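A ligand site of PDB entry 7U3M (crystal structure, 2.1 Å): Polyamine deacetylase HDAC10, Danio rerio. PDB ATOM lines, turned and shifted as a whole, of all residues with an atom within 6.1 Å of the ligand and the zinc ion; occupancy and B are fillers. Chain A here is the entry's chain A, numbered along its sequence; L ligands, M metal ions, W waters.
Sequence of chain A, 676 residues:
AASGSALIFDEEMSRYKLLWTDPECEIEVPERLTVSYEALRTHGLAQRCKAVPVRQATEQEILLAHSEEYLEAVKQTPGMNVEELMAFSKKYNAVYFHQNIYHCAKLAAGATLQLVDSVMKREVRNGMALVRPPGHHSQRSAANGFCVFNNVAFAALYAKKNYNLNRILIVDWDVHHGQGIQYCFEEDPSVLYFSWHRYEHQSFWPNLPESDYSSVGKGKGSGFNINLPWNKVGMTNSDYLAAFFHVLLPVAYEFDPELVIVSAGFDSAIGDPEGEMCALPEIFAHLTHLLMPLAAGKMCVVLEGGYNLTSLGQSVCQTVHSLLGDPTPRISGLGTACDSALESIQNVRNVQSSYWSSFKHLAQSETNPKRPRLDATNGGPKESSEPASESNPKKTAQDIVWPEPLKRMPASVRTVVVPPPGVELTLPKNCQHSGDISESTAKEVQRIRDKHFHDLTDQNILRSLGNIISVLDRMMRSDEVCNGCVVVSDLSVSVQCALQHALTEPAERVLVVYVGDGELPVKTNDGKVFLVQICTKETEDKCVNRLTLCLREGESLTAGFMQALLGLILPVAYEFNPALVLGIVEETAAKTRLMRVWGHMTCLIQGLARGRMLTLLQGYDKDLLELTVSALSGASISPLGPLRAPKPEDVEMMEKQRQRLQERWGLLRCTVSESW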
ATOM      1  N   PRO A  23       4.978  17.654  29.310  1.00  0.00           N
ATOM      2  CA  PRO A  23       4.717  16.266  28.873  1.00  0.00           C
ATOM      3  C   PRO A  23       4.644  16.120  27.366  1.00  0.00           C
ATOM      4  O   PRO A  23       4.924  15.033  26.858  1.00  0.00           O
ATOM      5  CB  PRO A  23       3.368  15.934  29.549  1.00  0.00           C
ATOM      6  CG  PRO A  23       3.231  16.942  30.663  1.00  0.00           C
ATOM      7  CD  PRO A  23       3.896  18.189  30.148  1.00  0.00           C
ATOM      8  N   GLU A  24       4.299  17.186  26.638  1.00  0.00           N
ATOM      9  CA  GLU A  24       4.226  17.118  25.175  1.00  0.00           C
ATOM     10  C   GLU A  24       5.595  16.956  24.515  1.00  0.00           C
ATOM     11  O   GLU A  24       5.648  16.459  23.380  1.00  0.00           O
ATOM     12  CB  GLU A  24       3.535  18.363  24.627  1.00  0.00           C
ATOM     13  CG  GLU A  24       2.185  18.625  25.276  1.00  0.00           C
ATOM     14  CD  GLU A  24       1.126  17.640  24.805  1.00  0.00           C
ATOM     15  OE1 GLU A  24       0.425  17.940  23.810  1.00  0.00           O
ATOM     16  OE2 GLU A  24       1.003  16.561  25.429  1.00  0.00           O
ATOM     17  N   CYS A  25       6.688  17.365  25.173  1.00  0.00           N
ATOM     18  CA  CYS A  25       8.032  17.276  24.589  1.00  0.00           C
ATOM     19  C   CYS A  25       8.998  16.386  25.332  1.00  0.00           C
ATOM     20  O   CYS A  25      10.161  16.295  24.897  1.00  0.00           O
ATOM     21  CB  CYS A  25       8.693  18.668  24.467  1.00  0.00           C
ATOM     22  SG  CYS A  25       7.787  20.009  23.623  1.00  0.00           S
ATOM     23  N   ILE A  27       9.719  13.420  25.329  1.00  0.00           N
ATOM     24  CA  ILE A  27      10.299  12.271  24.625  1.00  0.00           C
ATOM     25  C   ILE A  27      11.460  12.607  23.703  1.00  0.00           C
ATOM     26  O   ILE A  27      12.143  11.681  23.222  1.00  0.00           O
ATOM     27  CB  ILE A  27       9.247  11.565  23.748  1.00  0.00           C
ATOM     28  CG1 ILE A  27       8.612  12.587  22.810  1.00  0.00           C
ATOM     29  CG2 ILE A  27       8.210  10.847  24.603  1.00  0.00           C
ATOM     30  CD1 ILE A  27       7.835  11.957  21.722  1.00  0.00           C
ATOM     31  N   ALA A  94       4.268  22.262  20.266  1.00  0.00           N
ATOM     32  CA  ALA A  94       5.058  21.070  20.626  1.00  0.00           C
ATOM     33  C   ALA A  94       6.538  21.211  20.240  1.00  0.00           C
ATOM     34  O   ALA A  94       7.101  20.401  19.503  1.00  0.00           O
ATOM     35  CB  ALA A  94       4.441  19.813  20.005  1.00  0.00           C
ATOM     36  N   PRO A 134      15.229  17.406  14.692  1.00  0.00           N
ATOM     37  CA  PRO A 134      14.647  16.975  13.415  1.00  0.00           C
ATOM     38  C   PRO A 134      14.103  18.145  12.619  1.00  0.00           C
ATOM     39  O   PRO A 134      14.145  19.288  13.096  1.00  0.00           O
ATOM     40  CB  PRO A 134      13.530  16.025  13.854  1.00  0.00           C
ATOM     41  CG  PRO A 134      13.077  16.621  15.186  1.00  0.00           C
ATOM     42  CD  PRO A 134      14.360  17.087  15.843  1.00  0.00           C
ATOM     43  N   HIS A 136      11.157  17.889   9.739  1.00  0.00           N
ATOM     44  CA  HIS A 136      10.121  17.878   8.703  1.00  0.00           C
ATOM     45  C   HIS A 136       8.827  18.597   9.101  1.00  0.00           C
ATOM     46  O   HIS A 136       8.055  18.953   8.210  1.00  0.00           O
ATOM     47  CB  HIS A 136       9.859  16.434   8.233  1.00  0.00           C
ATOM     48  CG  HIS A 136       9.236  15.535   9.262  1.00  0.00           C
ATOM     49  ND1 HIS A 136       8.450  14.448   8.912  1.00  0.00           N
ATOM     50  CD2 HIS A 136       9.295  15.525  10.617  1.00  0.00           C
ATOM     51  CE1 HIS A 136       8.052  13.822  10.011  1.00  0.00           C
ATOM     52  NE2 HIS A 136       8.542  14.465  11.057  1.00  0.00           N
ATOM     53  N   HIS A 137       8.605  18.889  10.381  1.00  0.00           N
ATOM     54  CA  HIS A 137       7.467  19.698  10.797  1.00  0.00           C
ATOM     55  C   HIS A 137       7.722  21.200  10.691  1.00  0.00           C
ATOM     56  O   HIS A 137       6.756  21.983  10.726  1.00  0.00           O
ATOM     57  CB  HIS A 137       7.071  19.370  12.235  1.00  0.00           C
ATOM     58  CG  HIS A 137       6.642  17.956  12.417  1.00  0.00           C
ATOM     59  ND1 HIS A 137       5.828  17.304  11.515  1.00  0.00           N
ATOM     60  CD2 HIS A 137       6.929  17.048  13.381  1.00  0.00           C
ATOM     61  CE1 HIS A 137       5.644  16.054  11.906  1.00  0.00           C
ATOM     62  NE2 HIS A 137       6.294  15.876  13.041  1.00  0.00           N
ATOM     63  N   GLY A 145       6.733  20.777  16.284  1.00  0.00           N
ATOM     64  CA  GLY A 145       6.998  19.383  16.568  1.00  0.00           C
ATOM     65  C   GLY A 145       8.487  19.045  16.669  1.00  0.00           C
ATOM     66  O   GLY A 145       8.975  18.244  15.878  1.00  0.00           O
ATOM     67  N   PHE A 146       9.197  19.687  17.601  1.00  0.00           N
ATOM     68  CA  PHE A 146      10.631  19.476  17.864  1.00  0.00           C
ATOM     69  C   PHE A 146      11.550  20.021  16.780  1.00  0.00           C
ATOM     70  O   PHE A 146      12.761  20.044  16.976  1.00  0.00           O
ATOM     71  CB  PHE A 146      10.943  17.991  18.081  1.00  0.00           C
ATOM     72  CG  PHE A 146      10.109  17.353  19.132  1.00  0.00           C
ATOM     73  CD1 PHE A 146       9.739  18.069  20.252  1.00  0.00           C
ATOM     74  CD2 PHE A 146       9.677  16.049  19.002  1.00  0.00           C
ATOM     75  CE1 PHE A 146       8.948  17.491  21.225  1.00  0.00           C
ATOM     76  CE2 PHE A 146       8.901  15.461  19.976  1.00  0.00           C
ATOM     77  CZ  PHE A 146       8.522  16.186  21.088  1.00  0.00           C
ATOM     78  N   CYS A 147      10.986  20.478  15.657  1.00  0.00           N
ATOM     79  CA  CYS A 147      11.767  20.938  14.517  1.00  0.00           C
ATOM     80  C   CYS A 147      11.931  22.456  14.529  1.00  0.00           C
ATOM     81  O   CYS A 147      10.976  23.195  14.794  1.00  0.00           O
ATOM     82  CB  CYS A 147      11.096  20.528  13.200  1.00  0.00           C
ATOM     83  SG  CYS A 147      10.729  18.771  13.133  1.00  0.00           S
ATOM     84  N   ASP A 174       8.780   8.612   8.552  1.00  0.00           N
ATOM     85  CA  ASP A 174       8.406   8.973   9.918  1.00  0.00           C
ATOM     86  C   ASP A 174       6.917   8.702  10.125  1.00  0.00           C
ATOM     87  O   ASP A 174       6.126   8.776   9.188  1.00  0.00           O
ATOM     88  CB  ASP A 174       8.699  10.459  10.142  1.00  0.00           C
ATOM     89  CG  ASP A 174       8.635  10.855  11.589  1.00  0.00           C
ATOM     90  OD1 ASP A 174       9.705  10.933  12.216  1.00  0.00           O
ATOM     91  OD2 ASP A 174       7.515  11.121  12.093  1.00  0.00           O
ATOM     92  N   VAL A 175       6.536   8.395  11.372  1.00  0.00           N
ATOM     93  CA  VAL A 175       5.138   8.100  11.663  1.00  0.00           C
ATOM     94  C   VAL A 175       4.245   9.338  11.676  1.00  0.00           C
ATOM     95  O   VAL A 175       3.030   9.208  11.692  1.00  0.00           O
ATOM     96  CB  VAL A 175       4.993   7.350  13.003  1.00  0.00           C
ATOM     97  CG1 VAL A 175       4.932   8.351  14.185  1.00  0.00           C
ATOM     98  CG2 VAL A 175       3.742   6.459  12.967  1.00  0.00           C
ATOM     99  N   HIS A 176       4.827  10.536  11.684  1.00  0.00           N
ATOM    100  CA  HIS A 176       4.102  11.796  11.668  1.00  0.00           C
ATOM    101  C   HIS A 176       4.125  12.390  10.269  1.00  0.00           C
ATOM    102  O   HIS A 176       5.034  12.109   9.472  1.00  0.00           O
ATOM    103  CB  HIS A 176       4.709  12.789  12.664  1.00  0.00           C
ATOM    104  CG  HIS A 176       4.635  12.340  14.093  1.00  0.00           C
ATOM    105  ND1 HIS A 176       5.651  11.666  14.719  1.00  0.00           N
ATOM    106  CD2 HIS A 176       3.647  12.466  15.013  1.00  0.00           C
ATOM    107  CE1 HIS A 176       5.312  11.401  15.970  1.00  0.00           C
ATOM    108  NE2 HIS A 176       4.096  11.869  16.174  1.00  0.00           N
ATOM    109  N   PHE A 204      -5.225  12.579  15.228  1.00  0.00           N
ATOM    110  CA  PHE A 204      -3.837  12.489  15.690  1.00  0.00           C
ATOM    111  C   PHE A 204      -3.031  13.700  15.236  1.00  0.00           C
ATOM    112  O   PHE A 204      -3.157  14.160  14.098  1.00  0.00           O
ATOM    113  CB  PHE A 204      -3.160  11.208  15.210  1.00  0.00           C
ATOM    114  CG  PHE A 204      -1.895  10.896  15.954  1.00  0.00           C
ATOM    115  CD1 PHE A 204      -1.942  10.492  17.280  1.00  0.00           C
ATOM    116  CD2 PHE A 204      -0.658  11.020  15.327  1.00  0.00           C
ATOM    117  CE1 PHE A 204      -0.752  10.211  17.981  1.00  0.00           C
ATOM    118  CE2 PHE A 204       0.523  10.735  16.007  1.00  0.00           C
ATOM    119  CZ  PHE A 204       0.470  10.332  17.341  1.00  0.00           C
ATOM    120  N   TRP A 205      -2.200  14.211  16.145  1.00  0.00           N
ATOM    121  CA  TRP A 205      -1.309  15.333  15.873  1.00  0.00           C
ATOM    122  C   TRP A 205      -0.567  15.123  14.545  1.00  0.00           C
ATOM    123  O   TRP A 205      -0.085  14.010  14.272  1.00  0.00           O
ATOM    124  CB  TRP A 205      -0.323  15.477  17.048  1.00  0.00           C
ATOM    125  CG  TRP A 205       0.426  16.757  17.032  1.00  0.00           C
ATOM    126  CD1 TRP A 205       0.130  17.895  17.733  1.00  0.00           C
ATOM    127  CD2 TRP A 205       1.593  17.039  16.269  1.00  0.00           C
ATOM    128  NE1 TRP A 205       1.044  18.874  17.447  1.00  0.00           N
ATOM    129  CE2 TRP A 205       1.950  18.383  16.541  1.00  0.00           C
ATOM    130  CE3 TRP A 205       2.377  16.291  15.371  1.00  0.00           C
ATOM    131  CZ2 TRP A 205       3.072  18.987  15.966  1.00  0.00           C
ATOM    132  CZ3 TRP A 205       3.492  16.914  14.786  1.00  0.00           C
ATOM    133  CH2 TRP A 205       3.823  18.242  15.091  1.00  0.00           C
ATOM    134  N   GLY A 265      12.268   8.923   9.973  1.00  0.00           N
ATOM    135  CA  GLY A 265      11.871   8.810  11.353  1.00  0.00           C
ATOM    136  C   GLY A 265      11.554   7.351  11.615  1.00  0.00           C
ATOM    137  O   GLY A 265      10.869   6.693  10.828  1.00  0.00           O
ATOM    138  N   ASP A 267      10.066   6.436  14.471  1.00  0.00           N
ATOM    139  CA  ASP A 267       8.872   6.296  15.298  1.00  0.00           C
ATOM    140  C   ASP A 267       7.770   5.524  14.586  1.00  0.00           C
ATOM    141  O   ASP A 267       6.734   5.264  15.207  1.00  0.00           O
ATOM    142  CB  ASP A 267       8.362   7.660  15.753  1.00  0.00           C
ATOM    143  CG  ASP A 267       8.310   8.694  14.645  1.00  0.00           C
ATOM    144  OD1 ASP A 267       8.405   8.341  13.448  1.00  0.00           O
ATOM    145  OD2 ASP A 267       8.170   9.888  14.968  1.00  0.00           O
ATOM    146  N   GLU A 274       5.129   6.976  20.402  1.00  0.00           N
ATOM    147  CA  GLU A 274       4.343   7.927  19.622  1.00  0.00           C
ATOM    148  C   GLU A 274       3.585   7.251  18.491  1.00  0.00           C
ATOM    149  O   GLU A 274       2.419   7.586  18.247  1.00  0.00           O
ATOM    150  CB  GLU A 274       5.241   9.029  19.037  1.00  0.00           C
ATOM    151  CG  GLU A 274       5.420  10.188  19.954  1.00  0.00           C
ATOM    152  CD  GLU A 274       4.168  11.036  20.077  1.00  0.00           C
ATOM    153  OE1 GLU A 274       3.495  11.303  19.057  1.00  0.00           O
ATOM    154  OE2 GLU A 274       3.855  11.432  21.210  1.00  0.00           O
ATOM    155  N   GLU A 304      14.831  11.795  11.377  1.00  0.00           N
ATOM    156  CA  GLU A 304      13.808  12.662  11.941  1.00  0.00           C
ATOM    157  C   GLU A 304      13.527  12.182  13.353  1.00  0.00           C
ATOM    158  O   GLU A 304      14.265  12.543  14.293  1.00  0.00           O
ATOM    159  CB  GLU A 304      12.560  12.685  11.036  1.00  0.00           C
ATOM    160  CG  GLU A 304      12.838  13.192   9.605  1.00  0.00           C
ATOM    161  CD  GLU A 304      12.874  14.729   9.514  1.00  0.00           C
ATOM    162  OE1 GLU A 304      12.782  15.411  10.550  1.00  0.00           O
ATOM    163  OE2 GLU A 304      12.982  15.259   8.386  1.00  0.00           O
ATOM    164  N   GLY A 305      12.499  11.363  13.584  1.00  0.00           N
ATOM    165  CA  GLY A 305      12.097  10.956  14.906  1.00  0.00           C
ATOM    166  C   GLY A 305      12.443   9.508  15.215  1.00  0.00           C
ATOM    167  O   GLY A 305      13.218   8.855  14.525  1.00  0.00           O
ATOM    168  N   GLY A 306      11.835   9.014  16.299  1.00  0.00           N
ATOM    169  CA  GLY A 306      12.108   7.677  16.810  1.00  0.00           C
ATOM    170  C   GLY A 306      12.512   7.776  18.268  1.00  0.00           C
ATOM    171  O   GLY A 306      13.556   8.340  18.580  1.00  0.00           O
ATOM    172  N   TYR A 307      11.665   7.275  19.168  1.00  0.00           N
ATOM    173  CA  TYR A 307      11.792   7.580  20.582  1.00  0.00           C
ATOM    174  C   TYR A 307      11.947   6.376  21.495  1.00  0.00           C
ATOM    175  O   TYR A 307      12.196   6.567  22.682  1.00  0.00           O
ATOM    176  CB  TYR A 307      10.578   8.403  21.036  1.00  0.00           C
ATOM    177  CG  TYR A 307      10.423   9.578  20.127  1.00  0.00           C
ATOM    178  CD1 TYR A 307      11.246  10.687  20.292  1.00  0.00           C
ATOM    179  CD2 TYR A 307       9.534   9.546  19.063  1.00  0.00           C
ATOM    180  CE1 TYR A 307      11.162  11.753  19.447  1.00  0.00           C
ATOM    181  CE2 TYR A 307       9.428  10.630  18.209  1.00  0.00           C
ATOM    182  CZ  TYR A 307      10.239  11.724  18.406  1.00  0.00           C
ATOM    183  OH  TYR A 307      10.149  12.801  17.567  1.00  0.00           O
HETATM  184  C1  LIG L   1       6.521  14.614  17.393  1.00  0.00           C
HETATM  185  C2  LIG L   1       7.528  14.142  16.334  1.00  0.00           C
HETATM  186  C3  LIG L   1       2.122  15.114  21.780  1.00  0.00           C
HETATM  187  C4  LIG L   1       0.196  12.131  21.235  1.00  0.00           C
HETATM  188  C5  LIG L   1       1.118  13.483  19.752  1.00  0.00           C
HETATM  189  C6  LIG L   1       2.105  14.630  19.549  1.00  0.00           C
HETATM  190  C7  LIG L   1       3.696  15.912  20.424  1.00  0.00           C
HETATM  191  C8  LIG L   1       4.701  15.475  19.331  1.00  0.00           C
HETATM  192  C9  LIG L   1       5.515  14.321  19.547  1.00  0.00           C
HETATM  193  C10 LIG L   1       6.413  13.898  18.559  1.00  0.00           C
HETATM  194  C11 LIG L   1       5.718  15.795  17.157  1.00  0.00           C
HETATM  195  C12 LIG L   1       4.812  16.195  18.128  1.00  0.00           C
HETATM  196  C13 LIG L   1       1.133  13.971  22.063  1.00  0.00           C
HETATM  197  N1  LIG L   1       0.547  13.371  20.993  1.00  0.00           N
HETATM  198  N2  LIG L   1       2.863  14.916  20.651  1.00  0.00           N
HETATM  199  N3  LIG L   1       8.018  12.737  16.375  1.00  0.00           N
HETATM  200  O1  LIG L   1       7.894  14.851  15.503  1.00  0.00           O
HETATM  201  O2  LIG L   1       8.966  12.284  15.382  1.00  0.00           O
HETATM  202 ZN    ZN M   1       7.706  11.615  13.967  1.00  0.00          ZN
HETATM  203  O   HOH W   1       8.034  13.634  13.346  1.00  0.00           O
HETATM  204  O   HOH W   2      -1.031  16.287  21.184  1.00  0.00           O
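Water W1 lies within hydrogen-bond range of an oxygen (O1) of the ligand, a ring nitrogen (NE2) of His 136, a ring nitrogen (NE2) of His 137 and the side-chain carboxylate of Asp 174.
The nearest printed residue that does not touch the zinc ion is His 136 (4.2 Å).
N of Phe 146 lies within hydrogen-bond range of O of Ala 94 (2.9 Å).
The side-chain carboxylate of Asp 174 is in hydrogen-bond range of the backbone NH of Gly 305.
N of His 137 lies within hydrogen-bond range of SG of Cys 147, at 3.5 Å.
A ring nitrogen (NE2) of His 176 sits at hydrogen-bond distance from the side-chain carboxylate of Glu 274, 3.0 Å away.
The backbone carbonyl oxygen of Ala 94 sits close to the backbone NH of Gly 145, at 3.3 Å.
A ring nitrogen (NE2) of His 137 sits at hydrogen-bond distance from a ring nitrogen (NE2) of His 136.
The backbone carbonyl oxygen (O) of Gly 145 sits at hydrogen-bond distance from the side-chain sulfur (SG) of Cys 147 (3.3 Å).
OD1 of Asp 267 is in hydrogen-bond range of N of Val 175 (2.8 Å).
Glu 24 touches the ligand.
Ile 27 touches the ligand.
CB of Ala 94 touches C7 of the ligand, at 3.99 Å.
O of Gly 145 touches O1 of the ligand, at 3.6 Å.
CE2 of Phe 146 touches C10 of the ligand (3.3 Å).
Phe 204 touches the ligand (CE1 to C4, 3.9 Å).
Trp 205 touches the ligand.
CA of Gly 305 touches O2 of the ligand (3.4 Å).
Hydrophobic or aromatic side chains that line the ligand: Ile 27, Ala 94, His 137, Phe 146, His 176, Phe 204, Trp 205 and Tyr 307.
Of the 23 residues printed, 14 come within 4 Å of the ligand.
A nitrogen (N3) of the ligand is in hydrogen-bond range of the side-chain hydroxyl (OH) of Tyr 307, 2.4 Å away.
A nitrogen (N2) of the ligand is in salt-bridge range of the side-chain carboxylate (OE2) of Glu 274, at 3.7 Å.
A ring nitrogen (NE2) of His 137 is in hydrogen-bond range of an oxygen (O1) of the ligand, at 3.1 Å.
The zinc ion is bound by the side-chain carboxylate of Asp 174 (1.9 Å), an oxygen (O2) of the ligand (2.0 Å), the side-chain carboxylate of Asp 267 (2.0 Å), water W1 (2.1 Å) and a ring nitrogen (ND1) of His 176 (2.2 Å).
Slightly farther from the zinc ion lies OD1 of Asp 174 (2.7 Å).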
